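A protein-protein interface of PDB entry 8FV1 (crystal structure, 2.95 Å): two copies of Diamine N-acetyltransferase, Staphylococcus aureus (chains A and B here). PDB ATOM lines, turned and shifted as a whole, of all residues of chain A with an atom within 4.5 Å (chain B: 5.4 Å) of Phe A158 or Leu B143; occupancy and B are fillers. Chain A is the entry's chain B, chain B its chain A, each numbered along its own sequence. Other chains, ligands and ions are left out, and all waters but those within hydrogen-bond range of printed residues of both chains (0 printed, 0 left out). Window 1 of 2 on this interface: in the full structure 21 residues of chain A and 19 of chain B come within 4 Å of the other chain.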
ATOM      1  N   LYS A 116      19.009  20.673  18.182  1.00  0.00           N
ATOM      2  CA  LYS A 116      17.958  20.876  19.171  1.00  0.00           C
ATOM      3  C   LYS A 116      18.021  22.284  19.747  1.00  0.00           C
ATOM      4  O   LYS A 116      19.085  22.737  20.178  1.00  0.00           O
ATOM      5  CB  LYS A 116      18.078  19.840  20.292  1.00  0.00           C
ATOM      6  CG  LYS A 116      17.121  20.059  21.453  1.00  0.00           C
ATOM      7  CD  LYS A 116      17.314  19.005  22.531  1.00  0.00           C
ATOM      8  CE  LYS A 116      16.347  19.211  23.684  1.00  0.00           C
ATOM      9  NZ  LYS A 116      16.518  18.182  24.744  1.00  0.00           N
ATOM     10  N   TYR A 118      16.310  25.003  22.656  1.00  0.00           N
ATOM     11  CA  TYR A 118      15.613  24.950  23.933  1.00  0.00           C
ATOM     12  C   TYR A 118      15.464  26.361  24.483  1.00  0.00           C
ATOM     13  O   TYR A 118      16.056  27.317  23.978  1.00  0.00           O
ATOM     14  CB  TYR A 118      16.340  24.042  24.936  1.00  0.00           C
ATOM     15  CG  TYR A 118      17.724  24.508  25.322  1.00  0.00           C
ATOM     16  CD1 TYR A 118      18.836  24.141  24.576  1.00  0.00           C
ATOM     17  CD2 TYR A 118      17.922  25.308  26.441  1.00  0.00           C
ATOM     18  CE1 TYR A 118      20.104  24.562  24.927  1.00  0.00           C
ATOM     19  CE2 TYR A 118      19.187  25.731  26.802  1.00  0.00           C
ATOM     20  CZ  TYR A 118      20.274  25.357  26.041  1.00  0.00           C
ATOM     21  OH  TYR A 118      21.535  25.778  26.396  1.00  0.00           O
ATOM     22  N   LEU A 119      14.647  26.477  25.527  1.00  0.00           N
ATOM     23  CA  LEU A 119      14.345  27.770  26.120  1.00  0.00           C
ATOM     24  C   LEU A 119      13.773  27.560  27.515  1.00  0.00           C
ATOM     25  O   LEU A 119      13.264  26.484  27.849  1.00  0.00           O
ATOM     26  CB  LEU A 119      13.361  28.568  25.255  1.00  0.00           C
ATOM     27  CG  LEU A 119      11.914  28.069  25.209  1.00  0.00           C
ATOM     28  CD1 LEU A 119      11.077  28.647  26.347  1.00  0.00           C
ATOM     29  CD2 LEU A 119      11.278  28.391  23.862  1.00  0.00           C
ATOM     30  N   TYR A 120      13.867  28.615  28.319  1.00  0.00           N
ATOM     31  CA  TYR A 120      13.278  28.673  29.648  1.00  0.00           C
ATOM     32  C   TYR A 120      12.176  29.723  29.641  1.00  0.00           C
ATOM     33  O   TYR A 120      12.402  30.858  29.208  1.00  0.00           O
ATOM     34  CB  TYR A 120      14.328  29.025  30.704  1.00  0.00           C
ATOM     35  CG  TYR A 120      15.510  28.082  30.751  1.00  0.00           C
ATOM     36  CD1 TYR A 120      16.513  28.148  29.792  1.00  0.00           C
ATOM     37  CD2 TYR A 120      15.631  27.138  31.761  1.00  0.00           C
ATOM     38  CE1 TYR A 120      17.596  27.291  29.833  1.00  0.00           C
ATOM     39  CE2 TYR A 120      16.711  26.278  31.810  1.00  0.00           C
ATOM     40  CZ  TYR A 120      17.691  26.359  30.845  1.00  0.00           C
ATOM     41  OH  TYR A 120      18.768  25.506  30.889  1.00  0.00           O
ATOM     42  N   LYS A 138       8.087  21.514  23.001  1.00  0.00           N
ATOM     43  CA  LYS A 138       7.389  20.685  23.970  1.00  0.00           C
ATOM     44  C   LYS A 138       8.010  20.883  25.346  1.00  0.00           C
ATOM     45  O   LYS A 138       9.237  20.911  25.485  1.00  0.00           O
ATOM     46  CB  LYS A 138       7.455  19.204  23.584  1.00  0.00           C
ATOM     47  CG  LYS A 138       7.146  18.924  22.124  1.00  0.00           C
ATOM     48  CD  LYS A 138       7.001  17.432  21.867  1.00  0.00           C
ATOM     49  CE  LYS A 138       7.243  17.099  20.403  1.00  0.00           C
ATOM     50  NZ  LYS A 138       6.826  15.711  20.062  1.00  0.00           N
ATOM     51  N   THR A 139       7.160  21.018  26.360  1.00  0.00           N
ATOM     52  CA  THR A 139       7.621  21.202  27.735  1.00  0.00           C
ATOM     53  C   THR A 139       8.335  19.934  28.186  1.00  0.00           C
ATOM     54  O   THR A 139       7.698  18.934  28.525  1.00  0.00           O
ATOM     55  CB  THR A 139       6.451  21.529  28.653  1.00  0.00           C
ATOM     56  OG1 THR A 139       5.836  22.753  28.233  1.00  0.00           O
ATOM     57  CG2 THR A 139       6.925  21.669  30.095  1.00  0.00           C
ATOM     58  N   GLU A 140       9.667  19.972  28.196  1.00  0.00           N
ATOM     59  CA  GLU A 140      10.453  18.818  28.609  1.00  0.00           C
ATOM     60  C   GLU A 140      10.754  18.797  30.101  1.00  0.00           C
ATOM     61  O   GLU A 140      11.118  17.738  30.625  1.00  0.00           O
ATOM     62  CB  GLU A 140      11.774  18.765  27.834  1.00  0.00           C
ATOM     63  CG  GLU A 140      11.704  17.947  26.556  1.00  0.00           C
ATOM     64  CD  GLU A 140      13.060  17.764  25.903  1.00  0.00           C
ATOM     65  OE1 GLU A 140      14.002  18.495  26.275  1.00  0.00           O
ATOM     66  OE2 GLU A 140      13.182  16.889  25.020  1.00  0.00           O
ATOM     67  N   GLY A 141      10.621  19.922  30.796  1.00  0.00           N
ATOM     68  CA  GLY A 141      10.878  19.930  32.224  1.00  0.00           C
ATOM     69  C   GLY A 141      10.158  21.052  32.931  1.00  0.00           C
ATOM     70  O   GLY A 141       9.867  22.094  32.339  1.00  0.00           O
ATOM     71  N   ALA A 156       9.711  27.295  36.197  1.00  0.00           N
ATOM     72  CA  ALA A 156       9.933  27.566  34.786  1.00  0.00           C
ATOM     73  C   ALA A 156       9.822  26.286  33.975  1.00  0.00           C
ATOM     74  O   ALA A 156      10.330  25.236  34.372  1.00  0.00           O
ATOM     75  CB  ALA A 156      11.307  28.211  34.555  1.00  0.00           C
ATOM     76  N   TYR A 157       9.151  26.389  32.832  1.00  0.00           N
ATOM     77  CA  TYR A 157       9.155  25.322  31.845  1.00  0.00           C
ATOM     78  C   TYR A 157      10.456  25.382  31.051  1.00  0.00           C
ATOM     79  O   TYR A 157      10.777  26.415  30.445  1.00  0.00           O
ATOM     80  CB  TYR A 157       7.962  25.439  30.900  1.00  0.00           C
ATOM     81  CG  TYR A 157       6.618  25.064  31.489  1.00  0.00           C
ATOM     82  CD1 TYR A 157       6.514  24.465  32.738  1.00  0.00           C
ATOM     83  CD2 TYR A 157       5.448  25.303  30.781  1.00  0.00           C
ATOM     84  CE1 TYR A 157       5.282  24.123  33.264  1.00  0.00           C
ATOM     85  CE2 TYR A 157       4.215  24.966  31.299  1.00  0.00           C
ATOM     86  CZ  TYR A 157       4.137  24.376  32.539  1.00  0.00           C
ATOM     87  OH  TYR A 157       2.909  24.038  33.059  1.00  0.00           O
ATOM     88  N   PHE A 158      11.213  24.290  31.086  1.00  0.00           N
ATOM     89  CA  PHE A 158      12.278  24.029  30.126  1.00  0.00           C
ATOM     90  C   PHE A 158      11.623  23.369  28.920  1.00  0.00           C
ATOM     91  O   PHE A 158      11.207  22.204  28.995  1.00  0.00           O
ATOM     92  CB  PHE A 158      13.358  23.134  30.729  1.00  0.00           C
ATOM     93  CG  PHE A 158      14.513  22.859  29.798  1.00  0.00           C
ATOM     94  CD1 PHE A 158      14.370  21.995  28.723  1.00  0.00           C
ATOM     95  CD2 PHE A 158      15.744  23.459  30.006  1.00  0.00           C
ATOM     96  CE1 PHE A 158      15.427  21.744  27.869  1.00  0.00           C
ATOM     97  CE2 PHE A 158      16.806  23.209  29.156  1.00  0.00           C
ATOM     98  CZ  PHE A 158      16.646  22.349  28.087  1.00  0.00           C
ATOM     99  N   MET A 159      11.509  24.114  27.825  1.00  0.00           N
ATOM    100  CA  MET A 159      10.902  23.633  26.594  1.00  0.00           C
ATOM    101  C   MET A 159      11.982  23.482  25.531  1.00  0.00           C
ATOM    102  O   MET A 159      13.056  24.080  25.624  1.00  0.00           O
ATOM    103  CB  MET A 159       9.812  24.594  26.109  1.00  0.00           C
ATOM    104  CG  MET A 159       8.783  24.947  27.175  1.00  0.00           C
ATOM    105  SD  MET A 159       7.529  26.104  26.591  1.00  0.00           S
ATOM    106  CE  MET A 159       6.757  25.146  25.290  1.00  0.00           C
ATOM    107  N   SER A 160      11.694  22.673  24.516  1.00  0.00           N
ATOM    108  CA  SER A 160      12.682  22.439  23.474  1.00  0.00           C
ATOM    109  C   SER A 160      12.013  21.867  22.235  1.00  0.00           C
ATOM    110  O   SER A 160      10.887  21.364  22.281  1.00  0.00           O
ATOM    111  CB  SER A 160      13.794  21.503  23.964  1.00  0.00           C
ATOM    112  OG  SER A 160      13.255  20.369  24.619  1.00  0.00           O
ATOM    113  N   TYR B 120      22.451  17.367  36.048  1.00  0.00           N
ATOM    114  CA  TYR B 120      22.110  16.586  34.866  1.00  0.00           C
ATOM    115  C   TYR B 120      22.735  15.204  35.003  1.00  0.00           C
ATOM    116  O   TYR B 120      23.908  15.089  35.377  1.00  0.00           O
ATOM    117  CB  TYR B 120      22.617  17.256  33.588  1.00  0.00           C
ATOM    118  CG  TYR B 120      22.133  18.671  33.375  1.00  0.00           C
ATOM    119  CD1 TYR B 120      22.646  19.720  34.125  1.00  0.00           C
ATOM    120  CD2 TYR B 120      21.179  18.962  32.409  1.00  0.00           C
ATOM    121  CE1 TYR B 120      22.214  21.016  33.931  1.00  0.00           C
ATOM    122  CE2 TYR B 120      20.741  20.255  32.206  1.00  0.00           C
ATOM    123  CZ  TYR B 120      21.262  21.278  32.969  1.00  0.00           C
ATOM    124  OH  TYR B 120      20.830  22.568  32.770  1.00  0.00           O
ATOM    125  N   GLY B 141      12.635  16.887  34.954  1.00  0.00           N
ATOM    126  CA  GLY B 141      12.512  16.937  33.513  1.00  0.00           C
ATOM    127  C   GLY B 141      13.433  15.923  32.875  1.00  0.00           C
ATOM    128  O   GLY B 141      14.385  15.436  33.495  1.00  0.00           O
ATOM    129  N   LEU B 142      13.126  15.608  31.618  1.00  0.00           N
ATOM    130  CA  LEU B 142      13.926  14.685  30.816  1.00  0.00           C
ATOM    131  C   LEU B 142      14.288  15.396  29.516  1.00  0.00           C
ATOM    132  O   LEU B 142      13.446  15.538  28.623  1.00  0.00           O
ATOM    133  CB  LEU B 142      13.178  13.383  30.545  1.00  0.00           C
ATOM    134  CG  LEU B 142      13.840  12.439  29.537  1.00  0.00           C
ATOM    135  CD1 LEU B 142      15.246  12.032  29.972  1.00  0.00           C
ATOM    136  CD2 LEU B 142      12.976  11.204  29.322  1.00  0.00           C
ATOM    137  N   LEU B 143      15.537  15.847  29.414  1.00  0.00           N
ATOM    138  CA  LEU B 143      16.030  16.471  28.193  1.00  0.00           C
ATOM    139  C   LEU B 143      16.470  15.373  27.234  1.00  0.00           C
ATOM    140  O   LEU B 143      17.381  14.599  27.545  1.00  0.00           O
ATOM    141  CB  LEU B 143      17.179  17.422  28.507  1.00  0.00           C
ATOM    142  CG  LEU B 143      16.954  18.310  29.732  1.00  0.00           C
ATOM    143  CD1 LEU B 143      18.015  19.393  29.798  1.00  0.00           C
ATOM    144  CD2 LEU B 143      15.557  18.914  29.722  1.00  0.00           C
ATOM    145  N   LYS B 144      15.812  15.291  26.083  1.00  0.00           N
ATOM    146  CA  LYS B 144      15.983  14.176  25.164  1.00  0.00           C
ATOM    147  C   LYS B 144      16.882  14.603  24.016  1.00  0.00           C
ATOM    148  O   LYS B 144      16.619  15.618  23.361  1.00  0.00           O
ATOM    149  CB  LYS B 144      14.626  13.704  24.637  1.00  0.00           C
ATOM    150  CG  LYS B 144      13.630  13.395  25.732  1.00  0.00           C
ATOM    151  CD  LYS B 144      12.357  12.822  25.156  1.00  0.00           C
ATOM    152  CE  LYS B 144      11.147  13.274  25.948  1.00  0.00           C
ATOM    153  NZ  LYS B 144       9.877  12.819  25.323  1.00  0.00           N
ATOM    154  N   GLU B 145      17.946  13.836  23.781  1.00  0.00           N
ATOM    155  CA  GLU B 145      18.927  14.183  22.756  1.00  0.00           C
ATOM    156  C   GLU B 145      19.541  15.548  23.046  1.00  0.00           C
ATOM    157  O   GLU B 145      19.888  16.305  22.136  1.00  0.00           O
ATOM    158  CB  GLU B 145      18.285  14.132  21.370  1.00  0.00           C
ATOM    159  CG  GLU B 145      17.523  12.831  21.155  1.00  0.00           C
ATOM    160  CD  GLU B 145      16.915  12.712  19.775  1.00  0.00           C
ATOM    161  OE1 GLU B 145      17.147  13.609  18.940  1.00  0.00           O
ATOM    162  OE2 GLU B 145      16.205  11.715  19.527  1.00  0.00           O
ATOM    163  N   GLN B 146      19.662  15.854  24.340  1.00  0.00           N
ATOM    164  CA  GLN B 146      20.293  17.079  24.806  1.00  0.00           C
ATOM    165  C   GLN B 146      21.813  17.001  24.792  1.00  0.00           C
ATOM    166  O   GLN B 146      22.469  18.048  24.737  1.00  0.00           O
ATOM    167  CB  GLN B 146      19.802  17.383  26.226  1.00  0.00           C
ATOM    168  CG  GLN B 146      20.376  18.639  26.845  1.00  0.00           C
ATOM    169  CD  GLN B 146      19.931  19.892  26.127  1.00  0.00           C
ATOM    170  OE1 GLN B 146      18.740  20.103  25.898  1.00  0.00           O
ATOM    171  NE2 GLN B 146      20.892  20.733  25.759  1.00  0.00           N
ATOM    172  N   LYS B 154      22.382  11.366  23.488  1.00  0.00           N
ATOM    173  CA  LYS B 154      21.848  10.809  24.722  1.00  0.00           C
ATOM    174  C   LYS B 154      20.982  11.820  25.464  1.00  0.00           C
ATOM    175  O   LYS B 154      21.201  13.041  25.403  1.00  0.00           O
ATOM    176  CB  LYS B 154      22.976  10.341  25.647  1.00  0.00           C
ATOM    177  CG  LYS B 154      24.002   9.466  24.971  1.00  0.00           C
ATOM    178  CD  LYS B 154      24.724   8.578  25.972  1.00  0.00           C
ATOM    179  CE  LYS B 154      23.851   7.410  26.423  1.00  0.00           C
ATOM    180  NZ  LYS B 154      24.605   6.412  27.235  1.00  0.00           N
ATOM    181  N   ASP B 155      19.992  11.278  26.169  1.00  0.00           N
ATOM    182  CA  ASP B 155      19.048  12.020  26.988  1.00  0.00           C
ATOM    183  C   ASP B 155      19.538  12.072  28.427  1.00  0.00           C
ATOM    184  O   ASP B 155      20.239  11.172  28.894  1.00  0.00           O
ATOM    185  CB  ASP B 155      17.675  11.351  26.927  1.00  0.00           C
ATOM    186  CG  ASP B 155      17.270  10.997  25.514  1.00  0.00           C
ATOM    187  OD1 ASP B 155      18.072  11.264  24.594  1.00  0.00           O
ATOM    188  OD2 ASP B 155      16.161  10.459  25.319  1.00  0.00           O
ATOM    189  N   ALA B 156      19.146  13.132  29.135  1.00  0.00           N
ATOM    190  CA  ALA B 156      19.573  13.333  30.512  1.00  0.00           C
ATOM    191  C   ALA B 156      18.395  13.775  31.366  1.00  0.00           C
ATOM    192  O   ALA B 156      17.555  14.562  30.924  1.00  0.00           O
ATOM    193  CB  ALA B 156      20.695  14.375  30.598  1.00  0.00           C
ATOM    194  N   TYR B 157      18.338  13.242  32.584  1.00  0.00           N
ATOM    195  CA  TYR B 157      17.374  13.685  33.579  1.00  0.00           C
ATOM    196  C   TYR B 157      17.926  14.899  34.313  1.00  0.00           C
ATOM    197  O   TYR B 157      19.098  14.920  34.711  1.00  0.00           O
ATOM    198  CB  TYR B 157      17.076  12.563  34.576  1.00  0.00           C
ATOM    199  CG  TYR B 157      16.268  11.421  34.004  1.00  0.00           C
ATOM    200  CD1 TYR B 157      14.960  11.615  33.579  1.00  0.00           C
ATOM    201  CD2 TYR B 157      16.807  10.143  33.906  1.00  0.00           C
ATOM    202  CE1 TYR B 157      14.213  10.573  33.060  1.00  0.00           C
ATOM    203  CE2 TYR B 157      16.069   9.094  33.389  1.00  0.00           C
ATOM    204  CZ  TYR B 157      14.772   9.313  32.966  1.00  0.00           C
ATOM    205  OH  TYR B 157      14.035   8.269  32.451  1.00  0.00           O
ATOM    206  N   PHE B 158      17.084  15.917  34.477  1.00  0.00           N
ATOM    207  CA  PHE B 158      17.410  17.116  35.243  1.00  0.00           C
ATOM    208  C   PHE B 158      16.848  16.919  36.649  1.00  0.00           C
ATOM    209  O   PHE B 158      15.664  17.161  36.890  1.00  0.00           O
ATOM    210  CB  PHE B 158      16.831  18.358  34.573  1.00  0.00           C
ATOM    211  CG  PHE B 158      17.168  19.645  35.272  1.00  0.00           C
ATOM    212  CD1 PHE B 158      16.490  20.031  36.417  1.00  0.00           C
ATOM    213  CD2 PHE B 158      18.151  20.481  34.769  1.00  0.00           C
ATOM    214  CE1 PHE B 158      16.796  21.217  37.054  1.00  0.00           C
ATOM    215  CE2 PHE B 158      18.459  21.669  35.400  1.00  0.00           C
ATOM    216  CZ  PHE B 158      17.779  22.039  36.542  1.00  0.00           C
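The backbone NH of Leu B142 lies within hydrogen-bond range of the backbone carbonyl oxygen of Glu A140, 3.1 Å away. O of Lys B144 sits at hydrogen-bond distance from NZ of Lys A116 (2.9 Å). N of Lys B144 is in hydrogen-bond range of OE2 of Glu A140 (3.3 Å). The side-chain amide oxygen (OE1) of Gln B146 lies within hydrogen-bond range of the side-chain amino group (NZ) of Lys A116 (3.2 Å).
N of Phe B158 lies within hydrogen-bond range of O of Gly B141 (2.9 Å). O of Leu B143 is in hydrogen-bond range of N of Ala B156 (2.8 Å). NZ of Lys A116 is in salt-bridge range of OE1 of Glu A140, 3.0 Å away. The backbone NH of Glu A140 sits at hydrogen-bond distance from the backbone carbonyl oxygen of Phe A158, at 2.8 Å. The side-chain carboxylate (OE1) of Glu A140 is in hydrogen-bond range of the side-chain hydroxyl (OG) of Ser A160, 2.6 Å away. The backbone carbonyl oxygen (O) of Gly A141 lies within hydrogen-bond range of the backbone NH (N) of Phe A158 (2.9 Å).
Among the printed residues, merely in contact across the chains: Glu A140 with Gly B141 (3.3 Å), Phe A158 with Leu B143 (3.4 Å), Glu A140 with Leu B143 (3.4 Å), Gly A141 with Gly B141 (3.6 Å), Lys A116 with Glu B145 (3.8 Å), Lys A116 with Leu B143 (3.8 Å), Phe A158 with Gln B146 (3.8 Å) and Tyr A118 with Gln B146 (3.997 Å).
Phe A158 touches just these residues of chain B: Leu B143 (3.4 Å) and Gln B146 (3.8 Å). Leu B143 touches just these residues of chain A: Lys A116 (3.8 Å), Glu A140 (3.4 Å) and Phe A158 (3.4 Å). Printed residues of chain B within 4 Å of Gly A141: Gly B141 (3.6 Å). Printed residues of chain B within 4 Å of Tyr A118: Gln B146. Printed residues of chain B within 4 Å of Glu A140: Gly B141 (3.3 Å), Leu B142 (3.1 Å), Leu B143 (3.4 Å) and Lys B144 (3.3 Å). Of the printed residues of chain A, Leu B142 touches Glu A140.
Of the 12 printed residues of chain B, 6 touch a printed residue of chain A. Printed residues of chain B that touch a printed residue of chain A: Gly B141, Leu B142, Leu B143, Lys B144, Glu B145 and Gln B146. Hydrophobic or aromatic side chains of chain B that line the printed part of chain A: Leu B143. Hydrophobic or aromatic side chains of chain A within 4 Å of the printed part of chain B: Tyr A118 and Phe A158.
Gly A141 touches its own counterpart, Gly B141.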
